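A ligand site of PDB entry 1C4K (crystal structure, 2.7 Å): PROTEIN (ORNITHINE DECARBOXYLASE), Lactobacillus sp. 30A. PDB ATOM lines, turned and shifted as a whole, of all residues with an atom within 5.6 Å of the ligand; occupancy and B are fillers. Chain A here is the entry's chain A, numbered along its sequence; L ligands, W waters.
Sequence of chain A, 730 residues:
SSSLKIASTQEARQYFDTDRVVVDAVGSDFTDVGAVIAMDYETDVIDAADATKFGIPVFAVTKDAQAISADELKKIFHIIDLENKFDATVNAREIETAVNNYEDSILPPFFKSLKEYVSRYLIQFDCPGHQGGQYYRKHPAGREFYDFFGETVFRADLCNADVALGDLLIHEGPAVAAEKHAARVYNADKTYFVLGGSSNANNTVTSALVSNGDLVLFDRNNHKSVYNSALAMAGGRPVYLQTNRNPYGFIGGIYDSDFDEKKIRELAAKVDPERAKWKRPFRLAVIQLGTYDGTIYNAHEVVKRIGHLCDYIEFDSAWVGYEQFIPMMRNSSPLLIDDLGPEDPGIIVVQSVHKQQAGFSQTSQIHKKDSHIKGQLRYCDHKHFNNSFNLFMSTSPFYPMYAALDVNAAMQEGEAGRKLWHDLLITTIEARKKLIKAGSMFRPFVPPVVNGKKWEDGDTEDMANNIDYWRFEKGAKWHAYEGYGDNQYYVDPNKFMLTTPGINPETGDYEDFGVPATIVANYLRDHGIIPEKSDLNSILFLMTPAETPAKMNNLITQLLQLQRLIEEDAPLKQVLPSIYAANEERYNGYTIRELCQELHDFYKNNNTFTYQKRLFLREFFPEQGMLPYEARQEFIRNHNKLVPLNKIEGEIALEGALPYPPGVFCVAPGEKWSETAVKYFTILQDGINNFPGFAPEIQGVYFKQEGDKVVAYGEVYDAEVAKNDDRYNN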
ATOM      1  N   ILE A 170      22.264 -27.463  23.346  1.00  0.00           N
ATOM      2  CA  ILE A 170      21.751 -26.463  24.291  1.00  0.00           C
ATOM      3  C   ILE A 170      20.407 -25.913  23.800  1.00  0.00           C
ATOM      4  O   ILE A 170      20.034 -24.794  24.125  1.00  0.00           O
ATOM      5  CB  ILE A 170      22.753 -25.312  24.633  1.00  0.00           C
ATOM      6  CG1 ILE A 170      23.016 -24.415  23.420  1.00  0.00           C
ATOM      7  CG2 ILE A 170      24.035 -25.886  25.199  1.00  0.00           C
ATOM      8  CD1 ILE A 170      23.761 -23.159  23.748  1.00  0.00           C
ATOM      9  N   HIS A 171      19.782 -26.682  22.905  1.00  0.00           N
ATOM     10  CA  HIS A 171      18.479 -26.426  22.277  1.00  0.00           C
ATOM     11  C   HIS A 171      18.088 -25.042  21.758  1.00  0.00           C
ATOM     12  O   HIS A 171      17.245 -24.345  22.337  1.00  0.00           O
ATOM     13  CB  HIS A 171      17.385 -26.971  23.216  1.00  0.00           C
ATOM     14  CG  HIS A 171      17.699 -28.309  23.789  1.00  0.00           C
ATOM     15  ND1 HIS A 171      17.759 -29.457  23.023  1.00  0.00           N
ATOM     16  CD2 HIS A 171      18.052 -28.683  25.042  1.00  0.00           C
ATOM     17  CE1 HIS A 171      18.124 -30.460  23.772  1.00  0.00           C
ATOM     18  NE2 HIS A 171      18.316 -30.027  25.009  1.00  0.00           N
ATOM     19  N   GLU A 172      18.598 -24.711  20.575  1.00  0.00           N
ATOM     20  CA  GLU A 172      18.296 -23.431  19.961  1.00  0.00           C
ATOM     21  C   GLU A 172      17.929 -23.548  18.482  1.00  0.00           C
ATOM     22  O   GLU A 172      18.205 -24.558  17.866  1.00  0.00           O
ATOM     23  CB  GLU A 172      19.491 -22.479  20.139  1.00  0.00           C
ATOM     24  CG  GLU A 172      19.388 -21.632  21.376  1.00  0.00           C
ATOM     25  CD  GLU A 172      20.734 -21.214  21.966  1.00  0.00           C
ATOM     26  OE1 GLU A 172      21.792 -21.474  21.342  1.00  0.00           O
ATOM     27  OE2 GLU A 172      20.723 -20.640  23.070  1.00  0.00           O
ATOM     28  N   VAL A 176      15.052 -26.705  18.627  1.00  0.00           N
ATOM     29  CA  VAL A 176      14.173 -26.615  19.811  1.00  0.00           C
ATOM     30  C   VAL A 176      12.724 -26.421  19.378  1.00  0.00           C
ATOM     31  O   VAL A 176      11.811 -26.714  20.140  1.00  0.00           O
ATOM     32  CB  VAL A 176      14.616 -25.484  20.787  1.00  0.00           C
ATOM     33  CG1 VAL A 176      14.520 -24.137  20.140  1.00  0.00           C
ATOM     34  CG2 VAL A 176      13.839 -25.524  22.056  1.00  0.00           C
ATOM     35  N   GLU A 179      11.332 -29.862  19.005  1.00  0.00           N
ATOM     36  CA  GLU A 179      11.086 -30.443  20.332  1.00  0.00           C
ATOM     37  C   GLU A 179       9.907 -29.791  21.076  1.00  0.00           C
ATOM     38  O   GLU A 179       9.267 -30.441  21.917  1.00  0.00           O
ATOM     39  CB  GLU A 179      12.329 -30.380  21.198  1.00  0.00           C
ATOM     40  CG  GLU A 179      13.498 -31.152  20.685  1.00  0.00           C
ATOM     41  CD  GLU A 179      14.710 -31.041  21.586  1.00  0.00           C
ATOM     42  OE1 GLU A 179      15.295 -29.949  21.675  1.00  0.00           O
ATOM     43  OE2 GLU A 179      15.103 -32.058  22.196  1.00  0.00           O
ATOM     44  N   LYS A 180       9.667 -28.503  20.802  1.00  0.00           N
ATOM     45  CA  LYS A 180       8.564 -27.785  21.456  1.00  0.00           C
ATOM     46  C   LYS A 180       7.275 -28.188  20.769  1.00  0.00           C
ATOM     47  O   LYS A 180       6.222 -28.128  21.384  1.00  0.00           O
ATOM     48  CB  LYS A 180       8.755 -26.278  21.414  1.00  0.00           C
ATOM     49  CG  LYS A 180       9.703 -25.728  22.461  1.00  0.00           C
ATOM     50  CD  LYS A 180      10.194 -24.330  22.092  1.00  0.00           C
ATOM     51  CE  LYS A 180       9.848 -23.310  23.146  1.00  0.00           C
ATOM     52  NZ  LYS A 180       8.368 -23.265  23.394  1.00  0.00           N
ATOM     53  N   ALA A 183       6.429 -31.676  22.102  1.00  0.00           N
ATOM     54  CA  ALA A 183       5.987 -31.493  23.464  1.00  0.00           C
ATOM     55  C   ALA A 183       4.526 -31.119  23.514  1.00  0.00           C
ATOM     56  O   ALA A 183       3.888 -31.366  24.520  1.00  0.00           O
ATOM     57  CB  ALA A 183       6.806 -30.440  24.135  1.00  0.00           C
ATOM     58  N   ASP A 189       5.548 -31.030  29.191  1.00  0.00           N
ATOM     59  CA  ASP A 189       6.182 -29.743  29.428  1.00  0.00           C
ATOM     60  C   ASP A 189       7.322 -29.576  28.453  1.00  0.00           C
ATOM     61  O   ASP A 189       7.325 -28.633  27.688  1.00  0.00           O
ATOM     62  CB  ASP A 189       6.702 -29.629  30.844  1.00  0.00           C
ATOM     63  CG  ASP A 189       5.630 -29.827  31.878  1.00  0.00           C
ATOM     64  OD1 ASP A 189       4.456 -29.505  31.642  1.00  0.00           O
ATOM     65  OD2 ASP A 189       5.974 -30.305  32.978  1.00  0.00           O
ATOM     66  N   LYS A 190       8.272 -30.516  28.473  1.00  0.00           N
ATOM     67  CA  LYS A 190       9.419 -30.462  27.588  1.00  0.00           C
ATOM     68  C   LYS A 190       9.725 -31.832  26.994  1.00  0.00           C
ATOM     69  O   LYS A 190       9.515 -32.855  27.645  1.00  0.00           O
ATOM     70  CB  LYS A 190      10.666 -29.952  28.310  1.00  0.00           C
ATOM     71  CG  LYS A 190      10.725 -28.446  28.481  1.00  0.00           C
ATOM     72  CD  LYS A 190      12.069 -27.987  29.041  1.00  0.00           C
ATOM     73  CE  LYS A 190      12.094 -26.483  29.224  1.00  0.00           C
ATOM     74  NZ  LYS A 190      10.926 -26.074  30.052  1.00  0.00           N
ATOM     75  N   THR A 191      10.251 -31.829  25.768  1.00  0.00           N
ATOM     76  CA  THR A 191      10.612 -33.032  25.042  1.00  0.00           C
ATOM     77  C   THR A 191      12.083 -33.021  24.639  1.00  0.00           C
ATOM     78  O   THR A 191      12.558 -32.072  24.005  1.00  0.00           O
ATOM     79  CB  THR A 191       9.755 -33.221  23.799  1.00  0.00           C
ATOM     80  OG1 THR A 191       8.410 -33.459  24.205  1.00  0.00           O
ATOM     81  CG2 THR A 191      10.215 -34.427  22.975  1.00  0.00           C
ATOM     82  N   TYR A 192      12.795 -34.108  24.960  1.00  0.00           N
ATOM     83  CA  TYR A 192      14.205 -34.262  24.636  1.00  0.00           C
ATOM     84  C   TYR A 192      14.375 -35.356  23.582  1.00  0.00           C
ATOM     85  O   TYR A 192      13.884 -36.476  23.756  1.00  0.00           O
ATOM     86  CB  TYR A 192      14.991 -34.616  25.896  1.00  0.00           C
ATOM     87  CG  TYR A 192      14.894 -33.541  26.949  1.00  0.00           C
ATOM     88  CD1 TYR A 192      13.753 -33.442  27.770  1.00  0.00           C
ATOM     89  CD2 TYR A 192      15.920 -32.582  27.102  1.00  0.00           C
ATOM     90  CE1 TYR A 192      13.639 -32.403  28.734  1.00  0.00           C
ATOM     91  CE2 TYR A 192      15.822 -31.542  28.049  1.00  0.00           C
ATOM     92  CZ  TYR A 192      14.693 -31.462  28.862  1.00  0.00           C
ATOM     93  OH  TYR A 192      14.627 -30.462  29.806  1.00  0.00           O
ATOM     94  N   LYS A 368       8.910 -34.867  29.469  1.00  0.00           N
ATOM     95  CA  LYS A 368       8.955 -34.453  30.862  1.00  0.00           C
ATOM     96  C   LYS A 368       7.668 -33.758  31.245  1.00  0.00           C
ATOM     97  O   LYS A 368       7.288 -32.790  30.626  1.00  0.00           O
ATOM     98  CB  LYS A 368      10.150 -33.511  31.040  1.00  0.00           C
ATOM     99  CG  LYS A 368      10.765 -33.494  32.415  1.00  0.00           C
ATOM    100  CD  LYS A 368      12.195 -32.996  32.325  1.00  0.00           C
ATOM    101  CE  LYS A 368      12.740 -32.629  33.678  1.00  0.00           C
ATOM    102  NZ  LYS A 368      12.116 -31.373  34.189  1.00  0.00           N
ATOM    103  N   LYS A 374       6.970 -27.647  40.433  1.00  0.00           N
ATOM    104  CA  LYS A 374       8.020 -26.650  40.158  1.00  0.00           C
ATOM    105  C   LYS A 374       8.759 -25.899  41.281  1.00  0.00           C
ATOM    106  O   LYS A 374       9.937 -25.595  41.133  1.00  0.00           O
ATOM    107  CB  LYS A 374       7.492 -25.629  39.137  1.00  0.00           C
ATOM    108  CG  LYS A 374       8.489 -25.161  38.064  1.00  0.00           C
ATOM    109  CD  LYS A 374       9.290 -23.938  38.489  1.00  0.00           C
ATOM    110  CE  LYS A 374      10.325 -23.540  37.434  1.00  0.00           C
ATOM    111  NZ  LYS A 374       9.749 -22.952  36.191  1.00  0.00           N
ATOM    112  N   TYR A 379      12.218 -31.169  42.618  1.00  0.00           N
ATOM    113  CA  TYR A 379      12.118 -30.822  41.205  1.00  0.00           C
ATOM    114  C   TYR A 379      13.443 -30.822  40.502  1.00  0.00           C
ATOM    115  O   TYR A 379      14.457 -30.441  41.060  1.00  0.00           O
ATOM    116  CB  TYR A 379      11.426 -29.481  41.057  1.00  0.00           C
ATOM    117  CG  TYR A 379      11.173 -29.017  39.628  1.00  0.00           C
ATOM    118  CD1 TYR A 379      10.238 -29.676  38.798  1.00  0.00           C
ATOM    119  CD2 TYR A 379      11.833 -27.879  39.107  1.00  0.00           C
ATOM    120  CE1 TYR A 379       9.977 -29.218  37.512  1.00  0.00           C
ATOM    121  CE2 TYR A 379      11.569 -27.422  37.830  1.00  0.00           C
ATOM    122  CZ  TYR A 379      10.646 -28.091  37.034  1.00  0.00           C
ATOM    123  OH  TYR A 379      10.391 -27.624  35.761  1.00  0.00           O
ATOM    124  N   CYS A 380      13.422 -31.272  39.249  1.00  0.00           N
ATOM    125  CA  CYS A 380      14.611 -31.330  38.442  1.00  0.00           C
ATOM    126  C   CYS A 380      14.366 -30.436  37.265  1.00  0.00           C
ATOM    127  O   CYS A 380      13.708 -30.843  36.326  1.00  0.00           O
ATOM    128  CB  CYS A 380      14.847 -32.768  37.992  1.00  0.00           C
ATOM    129  SG  CYS A 380      16.326 -33.003  37.008  1.00  0.00           S
ATOM    130  N   ASP A 381      14.923 -29.223  37.300  1.00  0.00           N
ATOM    131  CA  ASP A 381      14.732 -28.252  36.224  1.00  0.00           C
ATOM    132  C   ASP A 381      15.509 -28.531  34.930  1.00  0.00           C
ATOM    133  O   ASP A 381      16.413 -29.350  34.922  1.00  0.00           O
ATOM    134  CB  ASP A 381      15.042 -26.824  36.731  1.00  0.00           C
ATOM    135  CG  ASP A 381      16.473 -26.664  37.290  1.00  0.00           C
ATOM    136  OD1 ASP A 381      17.429 -27.260  36.747  1.00  0.00           O
ATOM    137  OD2 ASP A 381      16.647 -25.920  38.277  1.00  0.00           O
ATOM    138  N   HIS A 382      15.198 -27.774  33.883  1.00  0.00           N
ATOM    139  CA  HIS A 382      15.856 -27.926  32.604  1.00  0.00           C
ATOM    140  C   HIS A 382      17.391 -27.863  32.678  1.00  0.00           C
ATOM    141  O   HIS A 382      18.047 -28.547  31.912  1.00  0.00           O
ATOM    142  CB  HIS A 382      15.321 -26.876  31.603  1.00  0.00           C
ATOM    143  CG  HIS A 382      15.947 -26.955  30.245  1.00  0.00           C
ATOM    144  ND1 HIS A 382      15.677 -27.976  29.353  1.00  0.00           N
ATOM    145  CD2 HIS A 382      16.865 -26.167  29.633  1.00  0.00           C
ATOM    146  CE1 HIS A 382      16.393 -27.814  28.260  1.00  0.00           C
ATOM    147  NE2 HIS A 382      17.120 -26.721  28.399  1.00  0.00           N
ATOM    148  N   LYS A 383      17.952 -27.066  33.577  1.00  0.00           N
ATOM    149  CA  LYS A 383      19.406 -26.986  33.682  1.00  0.00           C
ATOM    150  C   LYS A 383      19.958 -28.324  34.144  1.00  0.00           C
ATOM    151  O   LYS A 383      20.879 -28.878  33.541  1.00  0.00           O
ATOM    152  CB  LYS A 383      19.823 -25.833  34.600  1.00  0.00           C
ATOM    153  CG  LYS A 383      19.230 -24.517  34.136  1.00  0.00           C
ATOM    154  CD  LYS A 383      19.564 -23.335  35.053  1.00  0.00           C
ATOM    155  CE  LYS A 383      18.549 -22.171  34.880  1.00  0.00           C
ATOM    156  NZ  LYS A 383      18.543 -21.534  33.528  1.00  0.00           N
ATOM    157  N   ASN A 386      19.178 -31.160  31.352  1.00  0.00           N
ATOM    158  CA  ASN A 386      19.998 -31.011  30.142  1.00  0.00           C
ATOM    159  C   ASN A 386      21.476 -31.346  30.368  1.00  0.00           C
ATOM    160  O   ASN A 386      22.180 -31.700  29.414  1.00  0.00           O
ATOM    161  CB  ASN A 386      19.848 -29.626  29.502  1.00  0.00           C
ATOM    162  CG  ASN A 386      20.059 -29.639  27.992  1.00  0.00           C
ATOM    163  OD1 ASN A 386      19.467 -30.454  27.280  1.00  0.00           O
ATOM    164  ND2 ASN A 386      20.881 -28.728  27.494  1.00  0.00           N
HETATM  165  P1  LIG L   1      12.383 -25.070  34.190  1.00  0.00           P
HETATM  166  O1  LIG L   1      10.964 -24.685  34.014  1.00  0.00           O
HETATM  167  O2  LIG L   1      12.727 -26.496  34.020  1.00  0.00           O
HETATM  168  O3  LIG L   1      12.830 -24.499  35.660  1.00  0.00           O
HETATM  169  O4  LIG L   1      13.395 -24.254  33.200  1.00  0.00           O
HETATM  170  P2  LIG L   1      12.767 -23.060  32.305  1.00  0.00           P
HETATM  171  O5  LIG L   1      12.156 -23.707  31.129  1.00  0.00           O
HETATM  172  O6  LIG L   1      11.891 -22.195  33.143  1.00  0.00           O
HETATM  173  O7  LIG L   1      13.943 -22.089  31.762  1.00  0.00           O
HETATM  174  P3  LIG L   1      15.435 -22.644  31.494  1.00  0.00           P
HETATM  175  O8  LIG L   1      16.296 -21.500  31.184  1.00  0.00           O
HETATM  176  O9  LIG L   1      15.862 -23.588  32.543  1.00  0.00           O
HETATM  177  O10 LIG L   1      15.113 -23.396  30.143  1.00  0.00           O
HETATM  178  C1  LIG L   1      14.718 -22.647  28.990  1.00  0.00           C
HETATM  179  C2  LIG L   1      15.391 -23.262  27.786  1.00  0.00           C
HETATM  180  O11 LIG L   1      14.984 -24.615  27.588  1.00  0.00           O
HETATM  181  C3  LIG L   1      15.035 -22.528  26.528  1.00  0.00           C
HETATM  182  O12 LIG L   1      15.896 -21.391  26.405  1.00  0.00           O
HETATM  183  C4  LIG L   1      15.267 -23.590  25.472  1.00  0.00           C
HETATM  184  O13 LIG L   1      16.577 -23.497  24.935  1.00  0.00           O
HETATM  185  C5  LIG L   1      15.011 -24.897  26.190  1.00  0.00           C
HETATM  186  N1  LIG L   1      13.711 -25.484  25.855  1.00  0.00           N
HETATM  187  C6  LIG L   1      12.473 -24.922  25.841  1.00  0.00           C
HETATM  188  N2  LIG L   1      11.531 -25.772  25.529  1.00  0.00           N
HETATM  189  C7  LIG L   1      12.200 -26.979  25.303  1.00  0.00           C
HETATM  190  C8  LIG L   1      11.709 -28.287  24.959  1.00  0.00           C
HETATM  191  O14 LIG L   1      10.562 -28.674  24.697  1.00  0.00           O
HETATM  192  N3  LIG L   1      12.756 -29.221  24.892  1.00  0.00           N
HETATM  193  C9  LIG L   1      14.079 -28.959  25.125  1.00  0.00           C
HETATM  194  N4  LIG L   1      14.917 -29.977  25.028  1.00  0.00           N
HETATM  195  N5  LIG L   1      14.529 -27.740  25.433  1.00  0.00           N
HETATM  196  C10 LIG L   1      13.539 -26.807  25.557  1.00  0.00           C
HETATM  197  O   HOH W   1       8.496 -26.775  25.556  1.00  0.00           O
HETATM  198  O   HOH W   2      10.908 -28.872  32.822  1.00  0.00           O
HETATM  199  O   HOH W   3      18.135 -25.172  26.614  1.00  0.00           O
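The backbone NH of Thr 191 lies within hydrogen-bond range of an oxygen (O14) of the ligand (3.3 Å).
The side-chain amino group of Lys 374 lies within salt-bridge range of an oxygen (O1) of the ligand (3.0 Å).
An oxygen (O5) of the ligand lies within salt-bridge range of the side-chain amino group (NZ) of Lys 190 (2.9 Å).
The backbone carbonyl oxygen (O) of Thr 191 is in hydrogen-bond range of a nitrogen (N3) of the ligand, at 3.0 Å.
O of His 171 lies within hydrogen-bond range of O13 of the ligand (2.8 Å).
NE2 of His 382 lies within hydrogen-bond range of O11 of the ligand (3.1 Å).
The side-chain hydroxyl (OH) of Tyr 379 lies within hydrogen-bond range of an oxygen (O2) of the ligand (3.1 Å).
The side-chain carboxylate of Glu 179 sits at hydrogen-bond distance from a nitrogen (N4) of the ligand (3.4 Å).
The side-chain amino group (NZ) of Lys 383 lies within salt-bridge range of an oxygen (O8) of the ligand, 3.2 Å away.
A nitrogen (N4) of the ligand sits close to a ring nitrogen (NE2) of His 171, 3.4 Å away.
The backbone NH (N) of His 382 is in hydrogen-bond range of an oxygen (O2) of the ligand, 2.8 Å away.
OG1 of Thr 191 sits close to N of Ala 183 (3.4 Å).
N of Lys 383 sits close to OD1 of Asp 381, 3.2 Å away.
A ring nitrogen (ND1) of His 171 sits at hydrogen-bond distance from the side-chain carboxylate (OE1) of Glu 179 (2.9 Å).
NE2 of His 171 is in hydrogen-bond range of OD1 of Asn 386 (2.6 Å).
The backbone carbonyl oxygen of Lys 190 is in hydrogen-bond range of the backbone NH of Lys 368, at 2.8 Å.
The side-chain hydroxyl (OH) of Tyr 192 is in hydrogen-bond range of a ring nitrogen (ND1) of His 382 (2.7 Å).
Ile 170 touches the ligand.
Val 176 touches the ligand.
Lys 180 touches the ligand.
CD2 of Tyr 192 touches N4 of the ligand, at 3.5 Å.
CB of Asp 381 touches O3 of the ligand, at 3.4 Å.
Within 4 Å of the ligand: Ile 170, His 171, Val 176, Glu 179, Lys 180, Lys 190, Thr 191, Tyr 192, Lys 374, Tyr 379, Asp 381, His 382 and Lys 383.
The nearest printed residue that does not touch the ligand is Ala 183 (4.2 Å).
Water W3 lies within hydrogen-bond range of NE2 of His 382 (2.6 Å), O13 of the ligand (2.8 Å) and O of Ile 170 (3.2 Å).
Water W1 lies within hydrogen-bond range of an oxygen (O14) of the ligand and the backbone carbonyl oxygen of Asp 189.
Water W2 lies within hydrogen-bond range of the side-chain amino group of Lys 368, an oxygen (O2) of the ligand and the side-chain hydroxyl of Tyr 379.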
